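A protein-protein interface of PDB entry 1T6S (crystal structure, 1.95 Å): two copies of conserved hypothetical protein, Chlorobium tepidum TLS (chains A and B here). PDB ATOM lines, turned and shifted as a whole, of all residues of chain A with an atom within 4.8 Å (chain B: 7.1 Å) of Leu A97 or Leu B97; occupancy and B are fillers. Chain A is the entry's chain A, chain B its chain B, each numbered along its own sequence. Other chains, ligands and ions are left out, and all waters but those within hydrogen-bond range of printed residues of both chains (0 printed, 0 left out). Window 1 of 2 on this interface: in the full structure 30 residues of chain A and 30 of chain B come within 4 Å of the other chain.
The guanidinium group of Arg A94 lies close to the indole nitrogen of Trp B105, at 3.1 Å.
The guanidinium group of Arg B128 lies close to the side-chain sulfur of Met B96.
Among the printed residues, merely in contact across the chains: Phe A160 with Met B96 (3.3 Å), Met A96 with Phe B160 (3.3 Å), Phe A160 with Phe B160 (3.5 Å), Phe A156 with Ser B93 (3.5 Å), Ser A93 with Phe B156 (3.5 Å), Ala A101 with Leu B97 (3.5 Å), Leu A97 with Ala B101 (3.5 Å), Leu A97 with Leu B100 (3.6 Å), Leu A100 with Leu B97 (3.6 Å), Phe A160 with Leu B97 (3.8 Å), Leu A97 with Phe B160 (3.8 Å), Leu A97 with Leu B97 (3.9 Å), Ala A104 with Ser B93 (3.97 Å) and Ser A93 with Ala B104 (3.98 Å).
Of chain B, only Leu B97 (3.9 Å), Leu B100 (3.6 Å), Ala B101 (3.5 Å) and Phe B160 (3.8 Å) come within 4 Å of Leu A97. Leu B97 touches just these residues of chain A: Leu A97, Leu A100, Ala A101 and Phe A160. Of the printed residues of chain A, Ala B104 touches Ser A93 (3.98 Å). Of the printed residues of chain A, Leu B100 touches Leu A97. Printed residues of chain B within 4 Å of Phe A156: Ser B93 (3.5 Å). Val B102 touches none of the printed residues of chain A. The nearest residue of chain A that does not touch Leu B97 is Phe A156 (4.1 Å). The nearest printed residue of chain A that does not touch Phe B156 is Leu A97 (4.1 Å).
Of the 21 printed residues of chain B, 9 touch a printed residue of chain A. Hydrophobic or aromatic side chains of chain B within 4 Å of the printed part of chain A: Met B96, Leu B97, Leu B100, Ala B101, Ala B104, Trp B105, Phe B156 and Phe B160. Along chain B the printed residues that touch a printed residue of chain A span positions 93 to 160. Of the 12 printed residues of chain A, 9 touch a printed residue of chain B. Hydrophobic or aromatic side chains of chain A within 4 Å of the printed part of chain B: Met A96, Leu A97, Leu A100, Ala A101, Ala A104, Phe A156 and Phe A160. Along chain A the printed residues that touch a printed residue of chain B span positions 93 to 160. Among the printed residues, 15 pairs touch across the chains.
Ser A93 touches Phe B156, and with the chains exchanged Phe A156 touches Ser B93. Leu A97 touches its own counterpart, Leu B97. Leu A97 touches Ala B101, and with the chains exchanged Ala A101 touches Leu B97. Leu A97 touches Phe B160, and with the chains exchanged Phe A160 touches Leu B97. Positions printed for both chains: 93, 94, 95, 96, 97, 98, 99, 100, 101, 104, 156 and 160.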
ATOM      1  N   SER A  93      25.844  31.270  12.520  1.00  0.00           N
ATOM      2  CA  SER A  93      25.183  30.898  11.273  1.00  0.00           C
ATOM      3  C   SER A  93      23.916  30.056  11.492  1.00  0.00           C
ATOM      4  O   SER A  93      22.855  30.358  10.941  1.00  0.00           O
ATOM      5  CB  SER A  93      26.144  30.113  10.374  1.00  0.00           C
ATOM      6  OG  SER A  93      27.159  30.954   9.853  1.00  0.00           O
ATOM      7  N   ARG A  94      24.029  28.997  12.287  1.00  0.00           N
ATOM      8  CA  ARG A  94      22.892  28.120  12.531  1.00  0.00           C
ATOM      9  C   ARG A  94      21.722  28.843  13.193  1.00  0.00           C
ATOM     10  O   ARG A  94      20.578  28.730  12.751  1.00  0.00           O
ATOM     11  CB  ARG A  94      23.312  26.926  13.397  1.00  0.00           C
ATOM     12  CG  ARG A  94      22.152  25.981  13.722  1.00  0.00           C
ATOM     13  CD  ARG A  94      22.580  24.718  14.469  1.00  0.00           C
ATOM     14  NE  ARG A  94      23.018  24.965  15.845  1.00  0.00           N
ATOM     15  CZ  ARG A  94      23.326  24.006  16.720  1.00  0.00           C
ATOM     16  NH1 ARG A  94      23.240  22.730  16.357  1.00  0.00           N
ATOM     17  NH2 ARG A  94      23.727  24.319  17.952  1.00  0.00           N
ATOM     18  N   SER A  95      22.011  29.580  14.258  1.00  0.00           N
ATOM     19  CA  SER A  95      20.966  30.284  14.972  1.00  0.00           C
ATOM     20  C   SER A  95      20.252  31.269  14.057  1.00  0.00           C
ATOM     21  O   SER A  95      19.023  31.294  14.022  1.00  0.00           O
ATOM     22  CB  SER A  95      21.532  30.991  16.219  1.00  0.00           C
ATOM     23  OG  SER A  95      22.480  31.988  15.889  1.00  0.00           O
ATOM     24  N   MET A  96      21.001  32.062  13.295  1.00  0.00           N
ATOM     25  CA  MET A  96      20.357  33.012  12.401  1.00  0.00           C
ATOM     26  C   MET A  96      19.472  32.309  11.381  1.00  0.00           C
ATOM     27  O   MET A  96      18.355  32.757  11.103  1.00  0.00           O
ATOM     28  CB  MET A  96      21.390  33.871  11.662  1.00  0.00           C
ATOM     29  CG  MET A  96      21.817  35.094  12.441  1.00  0.00           C
ATOM     30  SD  MET A  96      22.657  36.311  11.401  1.00  0.00           S
ATOM     31  CE  MET A  96      21.724  36.191   9.927  1.00  0.00           C
ATOM     32  N   LEU A  97      19.968  31.205  10.830  1.00  0.00           N
ATOM     33  CA  LEU A  97      19.212  30.451   9.838  1.00  0.00           C
ATOM     34  C   LEU A  97      17.939  29.807  10.395  1.00  0.00           C
ATOM     35  O   LEU A  97      16.884  29.855   9.753  1.00  0.00           O
ATOM     36  CB  LEU A  97      20.106  29.376   9.198  1.00  0.00           C
ATOM     37  CG  LEU A  97      21.172  29.957   8.255  1.00  0.00           C
ATOM     38  CD1 LEU A  97      21.967  28.817   7.640  1.00  0.00           C
ATOM     39  CD2 LEU A  97      20.512  30.774   7.152  1.00  0.00           C
ATOM     40  N   GLU A  98      18.041  29.198  11.578  1.00  0.00           N
ATOM     41  CA  GLU A  98      16.878  28.557  12.218  1.00  0.00           C
ATOM     42  C   GLU A  98      15.776  29.576  12.553  1.00  0.00           C
ATOM     43  O   GLU A  98      14.601  29.329  12.296  1.00  0.00           O
ATOM     44  CB  GLU A  98      17.289  27.825  13.513  1.00  0.00           C
ATOM     45  CG  GLU A  98      18.045  26.516  13.297  1.00  0.00           C
ATOM     46  CD  GLU A  98      18.382  25.771  14.603  1.00  0.00           C
ATOM     47  OE1 GLU A  98      18.920  24.641  14.524  1.00  0.00           O
ATOM     48  OE2 GLU A  98      18.117  26.311  15.705  1.00  0.00           O
ATOM     49  N   VAL A  99      16.162  30.709  13.132  1.00  0.00           N
ATOM     50  CA  VAL A  99      15.176  31.720  13.465  1.00  0.00           C
ATOM     51  C   VAL A  99      14.547  32.237  12.147  1.00  0.00           C
ATOM     52  O   VAL A  99      13.325  32.365  12.035  1.00  0.00           O
ATOM     53  CB  VAL A  99      15.807  32.890  14.290  1.00  0.00           C
ATOM     54  CG1 VAL A  99      14.805  34.043  14.443  1.00  0.00           C
ATOM     55  CG2 VAL A  99      16.223  32.383  15.671  1.00  0.00           C
ATOM     56  N   LEU A 100      15.382  32.499  11.141  1.00  0.00           N
ATOM     57  CA  LEU A 100      14.898  32.953   9.840  1.00  0.00           C
ATOM     58  C   LEU A 100      13.886  31.964   9.272  1.00  0.00           C
ATOM     59  O   LEU A 100      12.874  32.349   8.685  1.00  0.00           O
ATOM     60  CB  LEU A 100      16.041  33.058   8.828  1.00  0.00           C
ATOM     61  CG  LEU A 100      16.075  34.347   8.011  1.00  0.00           C
ATOM     62  CD1 LEU A 100      17.084  34.205   6.872  1.00  0.00           C
ATOM     63  CD2 LEU A 100      14.706  34.689   7.495  1.00  0.00           C
ATOM     64  N   ALA A 101      14.193  30.680   9.426  1.00  0.00           N
ATOM     65  CA  ALA A 101      13.343  29.601   8.952  1.00  0.00           C
ATOM     66  C   ALA A 101      12.000  29.614   9.677  1.00  0.00           C
ATOM     67  O   ALA A 101      10.960  29.424   9.053  1.00  0.00           O
ATOM     68  CB  ALA A 101      14.048  28.245   9.180  1.00  0.00           C
ATOM     69  N   ALA A 104      10.010  32.558   8.377  1.00  0.00           N
ATOM     70  CA  ALA A 104       9.533  32.260   7.035  1.00  0.00           C
ATOM     71  C   ALA A 104       8.301  31.391   7.091  1.00  0.00           C
ATOM     72  O   ALA A 104       7.348  31.604   6.336  1.00  0.00           O
ATOM     73  CB  ALA A 104      10.632  31.548   6.199  1.00  0.00           C
ATOM     74  N   PHE A 156      14.894  39.655   1.498  1.00  0.00           N
ATOM     75  CA  PHE A 156      15.226  38.247   1.732  1.00  0.00           C
ATOM     76  C   PHE A 156      14.840  37.426   0.502  1.00  0.00           C
ATOM     77  O   PHE A 156      15.632  36.635  -0.003  1.00  0.00           O
ATOM     78  CB  PHE A 156      14.462  37.673   2.940  1.00  0.00           C
ATOM     79  CG  PHE A 156      14.393  36.161   2.941  1.00  0.00           C
ATOM     80  CD1 PHE A 156      15.533  35.396   3.180  1.00  0.00           C
ATOM     81  CD2 PHE A 156      13.198  35.507   2.665  1.00  0.00           C
ATOM     82  CE1 PHE A 156      15.476  33.988   3.141  1.00  0.00           C
ATOM     83  CE2 PHE A 156      13.126  34.113   2.621  1.00  0.00           C
ATOM     84  CZ  PHE A 156      14.267  33.351   2.861  1.00  0.00           C
ATOM     85  N   PHE A 160      17.492  35.332  -1.943  1.00  0.00           N
ATOM     86  CA  PHE A 160      17.428  33.875  -2.097  1.00  0.00           C
ATOM     87  C   PHE A 160      16.757  33.382  -3.366  1.00  0.00           C
ATOM     88  O   PHE A 160      16.490  32.184  -3.510  1.00  0.00           O
ATOM     89  CB  PHE A 160      16.726  33.236  -0.904  1.00  0.00           C
ATOM     90  CG  PHE A 160      17.615  33.042   0.272  1.00  0.00           C
ATOM     91  CD1 PHE A 160      18.072  34.134   0.992  1.00  0.00           C
ATOM     92  CD2 PHE A 160      18.013  31.767   0.655  1.00  0.00           C
ATOM     93  CE1 PHE A 160      18.915  33.961   2.085  1.00  0.00           C
ATOM     94  CE2 PHE A 160      18.859  31.576   1.748  1.00  0.00           C
ATOM     95  CZ  PHE A 160      19.313  32.675   2.467  1.00  0.00           C
ATOM     96  N   ARG B  91       7.189  27.190   2.003  1.00  0.00           N
ATOM     97  CA  ARG B  91       7.779  25.852   1.939  1.00  0.00           C
ATOM     98  C   ARG B  91       9.172  25.916   1.306  1.00  0.00           C
ATOM     99  O   ARG B  91      10.125  25.360   1.843  1.00  0.00           O
ATOM    100  CB  ARG B  91       6.883  24.908   1.125  1.00  0.00           C
ATOM    101  CG  ARG B  91       5.570  24.509   1.828  1.00  0.00           C
ATOM    102  CD  ARG B  91       4.590  23.805   0.864  1.00  0.00           C
ATOM    103  NE  ARG B  91       5.090  22.528   0.360  1.00  0.00           N
ATOM    104  CZ  ARG B  91       4.449  21.762  -0.521  1.00  0.00           C
ATOM    105  NH1 ARG B  91       3.276  22.150  -1.003  1.00  0.00           N
ATOM    106  NH2 ARG B  91       4.982  20.604  -0.912  1.00  0.00           N
ATOM    107  N   LEU B  92       9.289  26.596   0.169  1.00  0.00           N
ATOM    108  CA  LEU B  92      10.584  26.731  -0.497  1.00  0.00           C
ATOM    109  C   LEU B  92      11.572  27.434   0.430  1.00  0.00           C
ATOM    110  O   LEU B  92      12.699  26.962   0.641  1.00  0.00           O
ATOM    111  CB  LEU B  92      10.438  27.522  -1.798  1.00  0.00           C
ATOM    112  CG  LEU B  92       9.598  26.828  -2.886  1.00  0.00           C
ATOM    113  CD1 LEU B  92       9.175  27.846  -3.945  1.00  0.00           C
ATOM    114  CD2 LEU B  92      10.401  25.686  -3.522  1.00  0.00           C
ATOM    115  N   SER B  93      11.158  28.569   0.983  1.00  0.00           N
ATOM    116  CA  SER B  93      12.011  29.314   1.907  1.00  0.00           C
ATOM    117  C   SER B  93      12.462  28.488   3.122  1.00  0.00           C
ATOM    118  O   SER B  93      13.655  28.449   3.457  1.00  0.00           O
ATOM    119  CB  SER B  93      11.291  30.570   2.411  1.00  0.00           C
ATOM    120  OG  SER B  93      11.151  31.531   1.371  1.00  0.00           O
ATOM    121  N   ARG B  94      11.518  27.836   3.789  1.00  0.00           N
ATOM    122  CA  ARG B  94      11.843  27.052   4.972  1.00  0.00           C
ATOM    123  C   ARG B  94      12.799  25.906   4.666  1.00  0.00           C
ATOM    124  O   ARG B  94      13.789  25.719   5.364  1.00  0.00           O
ATOM    125  CB  ARG B  94      10.564  26.494   5.608  1.00  0.00           C
ATOM    126  CG  ARG B  94      10.831  25.609   6.829  1.00  0.00           C
ATOM    127  CD  ARG B  94       9.560  25.162   7.550  1.00  0.00           C
ATOM    128  NE  ARG B  94       8.763  24.191   6.799  1.00  0.00           N
ATOM    129  CZ  ARG B  94       7.681  23.576   7.279  1.00  0.00           C
ATOM    130  NH1 ARG B  94       7.269  23.832   8.513  1.00  0.00           N
ATOM    131  NH2 ARG B  94       7.007  22.709   6.524  1.00  0.00           N
ATOM    132  N   SER B  95      12.491  25.136   3.628  1.00  0.00           N
ATOM    133  CA  SER B  95      13.326  24.005   3.272  1.00  0.00           C
ATOM    134  C   SER B  95      14.744  24.458   2.951  1.00  0.00           C
ATOM    135  O   SER B  95      15.700  23.872   3.451  1.00  0.00           O
ATOM    136  CB  SER B  95      12.713  23.222   2.098  1.00  0.00           C
ATOM    137  OG  SER B  95      12.642  23.995   0.912  1.00  0.00           O
ATOM    138  N   MET B  96      14.894  25.507   2.143  1.00  0.00           N
ATOM    139  CA  MET B  96      16.234  25.976   1.824  1.00  0.00           C
ATOM    140  C   MET B  96      16.989  26.409   3.073  1.00  0.00           C
ATOM    141  O   MET B  96      18.170  26.092   3.234  1.00  0.00           O
ATOM    142  CB  MET B  96      16.197  27.145   0.831  1.00  0.00           C
ATOM    143  CG  MET B  96      16.129  26.696  -0.611  1.00  0.00           C
ATOM    144  SD  MET B  96      16.552  28.020  -1.763  1.00  0.00           S
ATOM    145  CE  MET B  96      17.828  28.832  -0.877  1.00  0.00           C
ATOM    146  N   LEU B  97      16.301  27.122   3.960  1.00  0.00           N
ATOM    147  CA  LEU B  97      16.917  27.592   5.193  1.00  0.00           C
ATOM    148  C   LEU B  97      17.318  26.463   6.150  1.00  0.00           C
ATOM    149  O   LEU B  97      18.413  26.493   6.729  1.00  0.00           O
ATOM    150  CB  LEU B  97      15.987  28.580   5.912  1.00  0.00           C
ATOM    151  CG  LEU B  97      15.880  29.937   5.197  1.00  0.00           C
ATOM    152  CD1 LEU B  97      14.983  30.856   6.005  1.00  0.00           C
ATOM    153  CD2 LEU B  97      17.255  30.569   5.042  1.00  0.00           C
ATOM    154  N   GLU B  98      16.432  25.484   6.327  1.00  0.00           N
ATOM    155  CA  GLU B  98      16.724  24.340   7.218  1.00  0.00           C
ATOM    156  C   GLU B  98      17.920  23.516   6.718  1.00  0.00           C
ATOM    157  O   GLU B  98      18.787  23.143   7.504  1.00  0.00           O
ATOM    158  CB  GLU B  98      15.497  23.412   7.347  1.00  0.00           C
ATOM    159  CG  GLU B  98      14.369  23.953   8.215  1.00  0.00           C
ATOM    160  CD  GLU B  98      13.192  22.974   8.387  1.00  0.00           C
ATOM    161  OE1 GLU B  98      12.256  23.299   9.159  1.00  0.00           O
ATOM    162  OE2 GLU B  98      13.192  21.885   7.753  1.00  0.00           O
ATOM    163  N   VAL B  99      17.956  23.232   5.421  1.00  0.00           N
ATOM    164  CA  VAL B  99      19.065  22.468   4.878  1.00  0.00           C
ATOM    165  C   VAL B  99      20.357  23.309   5.033  1.00  0.00           C
ATOM    166  O   VAL B  99      21.399  22.804   5.469  1.00  0.00           O
ATOM    167  CB  VAL B  99      18.811  22.073   3.385  1.00  0.00           C
ATOM    168  CG1 VAL B  99      20.071  21.452   2.770  1.00  0.00           C
ATOM    169  CG2 VAL B  99      17.654  21.073   3.302  1.00  0.00           C
ATOM    170  N   LEU B 100      20.274  24.599   4.717  1.00  0.00           N
ATOM    171  CA  LEU B 100      21.420  25.493   4.859  1.00  0.00           C
ATOM    172  C   LEU B 100      21.939  25.463   6.290  1.00  0.00           C
ATOM    173  O   LEU B 100      23.147  25.469   6.538  1.00  0.00           O
ATOM    174  CB  LEU B 100      21.036  26.940   4.540  1.00  0.00           C
ATOM    175  CG  LEU B 100      21.997  27.677   3.611  1.00  0.00           C
ATOM    176  CD1 LEU B 100      21.662  29.163   3.596  1.00  0.00           C
ATOM    177  CD2 LEU B 100      23.430  27.445   4.024  1.00  0.00           C
ATOM    178  N   ALA B 101      21.002  25.457   7.230  1.00  0.00           N
ATOM    179  CA  ALA B 101      21.309  25.433   8.648  1.00  0.00           C
ATOM    180  C   ALA B 101      22.021  24.135   9.023  1.00  0.00           C
ATOM    181  O   ALA B 101      22.974  24.156   9.793  1.00  0.00           O
ATOM    182  CB  ALA B 101      20.007  25.576   9.463  1.00  0.00           C
ATOM    183  N   VAL B 102      21.542  23.011   8.487  1.00  0.00           N
ATOM    184  CA  VAL B 102      22.143  21.703   8.760  1.00  0.00           C
ATOM    185  C   VAL B 102      23.577  21.665   8.215  1.00  0.00           C
ATOM    186  O   VAL B 102      24.494  21.162   8.872  1.00  0.00           O
ATOM    187  CB  VAL B 102      21.302  20.549   8.138  1.00  0.00           C
ATOM    188  CG1 VAL B 102      21.992  19.201   8.374  1.00  0.00           C
ATOM    189  CG2 VAL B 102      19.902  20.521   8.763  1.00  0.00           C
ATOM    190  N   VAL B 103      23.776  22.214   7.021  1.00  0.00           N
ATOM    191  CA  VAL B 103      25.123  22.256   6.436  1.00  0.00           C
ATOM    192  C   VAL B 103      26.045  23.154   7.285  1.00  0.00           C
ATOM    193  O   VAL B 103      27.186  22.787   7.617  1.00  0.00           O
ATOM    194  CB  VAL B 103      25.084  22.760   4.977  1.00  0.00           C
ATOM    195  CG1 VAL B 103      26.532  22.821   4.388  1.00  0.00           C
ATOM    196  CG2 VAL B 103      24.211  21.822   4.152  1.00  0.00           C
ATOM    197  N   ALA B 104      25.542  24.327   7.650  1.00  0.00           N
ATOM    198  CA  ALA B 104      26.330  25.251   8.454  1.00  0.00           C
ATOM    199  C   ALA B 104      26.809  24.575   9.719  1.00  0.00           C
ATOM    200  O   ALA B 104      27.959  24.752  10.131  1.00  0.00           O
ATOM    201  CB  ALA B 104      25.502  26.505   8.824  1.00  0.00           C
ATOM    202  N   TRP B 105      25.942  23.781  10.336  1.00  0.00           N
ATOM    203  CA  TRP B 105      26.333  23.128  11.576  1.00  0.00           C
ATOM    204  C   TRP B 105      27.095  21.808  11.465  1.00  0.00           C
ATOM    205  O   TRP B 105      28.060  21.599  12.190  1.00  0.00           O
ATOM    206  CB  TRP B 105      25.100  22.931  12.462  1.00  0.00           C
ATOM    207  CG  TRP B 105      25.451  22.360  13.809  1.00  0.00           C
ATOM    208  CD1 TRP B 105      25.181  21.101  14.263  1.00  0.00           C
ATOM    209  CD2 TRP B 105      26.170  23.022  14.857  1.00  0.00           C
ATOM    210  NE1 TRP B 105      25.683  20.936  15.529  1.00  0.00           N
ATOM    211  CE2 TRP B 105      26.297  22.102  15.921  1.00  0.00           C
ATOM    212  CE3 TRP B 105      26.718  24.307  15.005  1.00  0.00           C
ATOM    213  CZ2 TRP B 105      26.949  22.422  17.114  1.00  0.00           C
ATOM    214  CZ3 TRP B 105      27.369  24.623  16.198  1.00  0.00           C
ATOM    215  CH2 TRP B 105      27.475  23.682  17.234  1.00  0.00           C
ATOM    216  N   SER B 125      16.818  20.802  -2.235  1.00  0.00           N
ATOM    217  CA  SER B 125      17.450  21.911  -1.538  1.00  0.00           C
ATOM    218  C   SER B 125      18.939  22.048  -1.810  1.00  0.00           C
ATOM    219  O   SER B 125      19.450  23.158  -1.957  1.00  0.00           O
ATOM    220  CB  SER B 125      17.188  21.805  -0.038  1.00  0.00           C
ATOM    221  OG  SER B 125      15.842  22.168   0.227  1.00  0.00           O
ATOM    222  N   ARG B 128      19.383  23.636  -5.141  1.00  0.00           N
ATOM    223  CA  ARG B 128      19.013  25.051  -5.079  1.00  0.00           C
ATOM    224  C   ARG B 128      20.103  25.878  -4.404  1.00  0.00           C
ATOM    225  O   ARG B 128      20.458  26.956  -4.879  1.00  0.00           O
ATOM    226  CB  ARG B 128      17.671  25.220  -4.349  1.00  0.00           C
ATOM    227  CG  ARG B 128      16.509  24.547  -5.054  1.00  0.00           C
ATOM    228  CD  ARG B 128      15.157  25.125  -4.616  1.00  0.00           C
ATOM    229  NE  ARG B 128      14.918  24.958  -3.180  1.00  0.00           N
ATOM    230  CZ  ARG B 128      14.418  23.865  -2.606  1.00  0.00           C
ATOM    231  NH1 ARG B 128      14.084  22.810  -3.343  1.00  0.00           N
ATOM    232  NH2 ARG B 128      14.263  23.830  -1.288  1.00  0.00           N
ATOM    233  N   LEU B 129      20.666  25.349  -3.324  1.00  0.00           N
ATOM    234  CA  LEU B 129      21.710  26.059  -2.593  1.00  0.00           C
ATOM    235  C   LEU B 129      23.006  26.132  -3.408  1.00  0.00           C
ATOM    236  O   LEU B 129      23.737  27.121  -3.336  1.00  0.00           O
ATOM    237  CB  LEU B 129      21.937  25.389  -1.230  1.00  0.00           C
ATOM    238  CG  LEU B 129      20.757  25.516  -0.240  1.00  0.00           C
ATOM    239  CD1 LEU B 129      21.024  24.709   1.012  1.00  0.00           C
ATOM    240  CD2 LEU B 129      20.568  27.000   0.123  1.00  0.00           C
ATOM    241  N   THR B 152      29.426  25.356   3.699  1.00  0.00           N
ATOM    242  CA  THR B 152      28.979  26.689   3.313  1.00  0.00           C
ATOM    243  C   THR B 152      30.120  27.397   2.566  1.00  0.00           C
ATOM    244  O   THR B 152      31.257  26.944   2.609  1.00  0.00           O
ATOM    245  CB  THR B 152      28.546  27.534   4.555  1.00  0.00           C
ATOM    246  OG1 THR B 152      29.569  27.467   5.554  1.00  0.00           O
ATOM    247  CG2 THR B 152      27.219  27.011   5.142  1.00  0.00           C
ATOM    248  N   PHE B 156      28.323  32.805   1.174  1.00  0.00           N
ATOM    249  CA  PHE B 156      27.268  32.750   2.192  1.00  0.00           C
ATOM    250  C   PHE B 156      27.670  33.619   3.383  1.00  0.00           C
ATOM    251  O   PHE B 156      26.893  34.442   3.854  1.00  0.00           O
ATOM    252  CB  PHE B 156      27.048  31.315   2.704  1.00  0.00           C
ATOM    253  CG  PHE B 156      26.348  31.259   4.049  1.00  0.00           C
ATOM    254  CD1 PHE B 156      25.004  31.609   4.167  1.00  0.00           C
ATOM    255  CD2 PHE B 156      27.045  30.888   5.194  1.00  0.00           C
ATOM    256  CE1 PHE B 156      24.359  31.592   5.418  1.00  0.00           C
ATOM    257  CE2 PHE B 156      26.420  30.866   6.443  1.00  0.00           C
ATOM    258  CZ  PHE B 156      25.071  31.219   6.556  1.00  0.00           C
ATOM    259  N   PHE B 160      25.663  37.028   4.698  1.00  0.00           N
ATOM    260  CA  PHE B 160      25.054  37.110   6.025  1.00  0.00           C
ATOM    261  C   PHE B 160      25.855  37.873   7.066  1.00  0.00           C
ATOM    262  O   PHE B 160      25.521  37.848   8.258  1.00  0.00           O
ATOM    263  CB  PHE B 160      24.760  35.719   6.572  1.00  0.00           C
ATOM    264  CG  PHE B 160      23.491  35.137   6.057  1.00  0.00           C
ATOM    265  CD1 PHE B 160      23.387  34.746   4.731  1.00  0.00           C
ATOM    266  CD2 PHE B 160      22.389  34.987   6.895  1.00  0.00           C
ATOM    267  CE1 PHE B 160      22.201  34.210   4.241  1.00  0.00           C
ATOM    268  CE2 PHE B 160      21.192  34.453   6.417  1.00  0.00           C
ATOM    269  CZ  PHE B 160      21.097  34.063   5.086  1.00  0.00           C
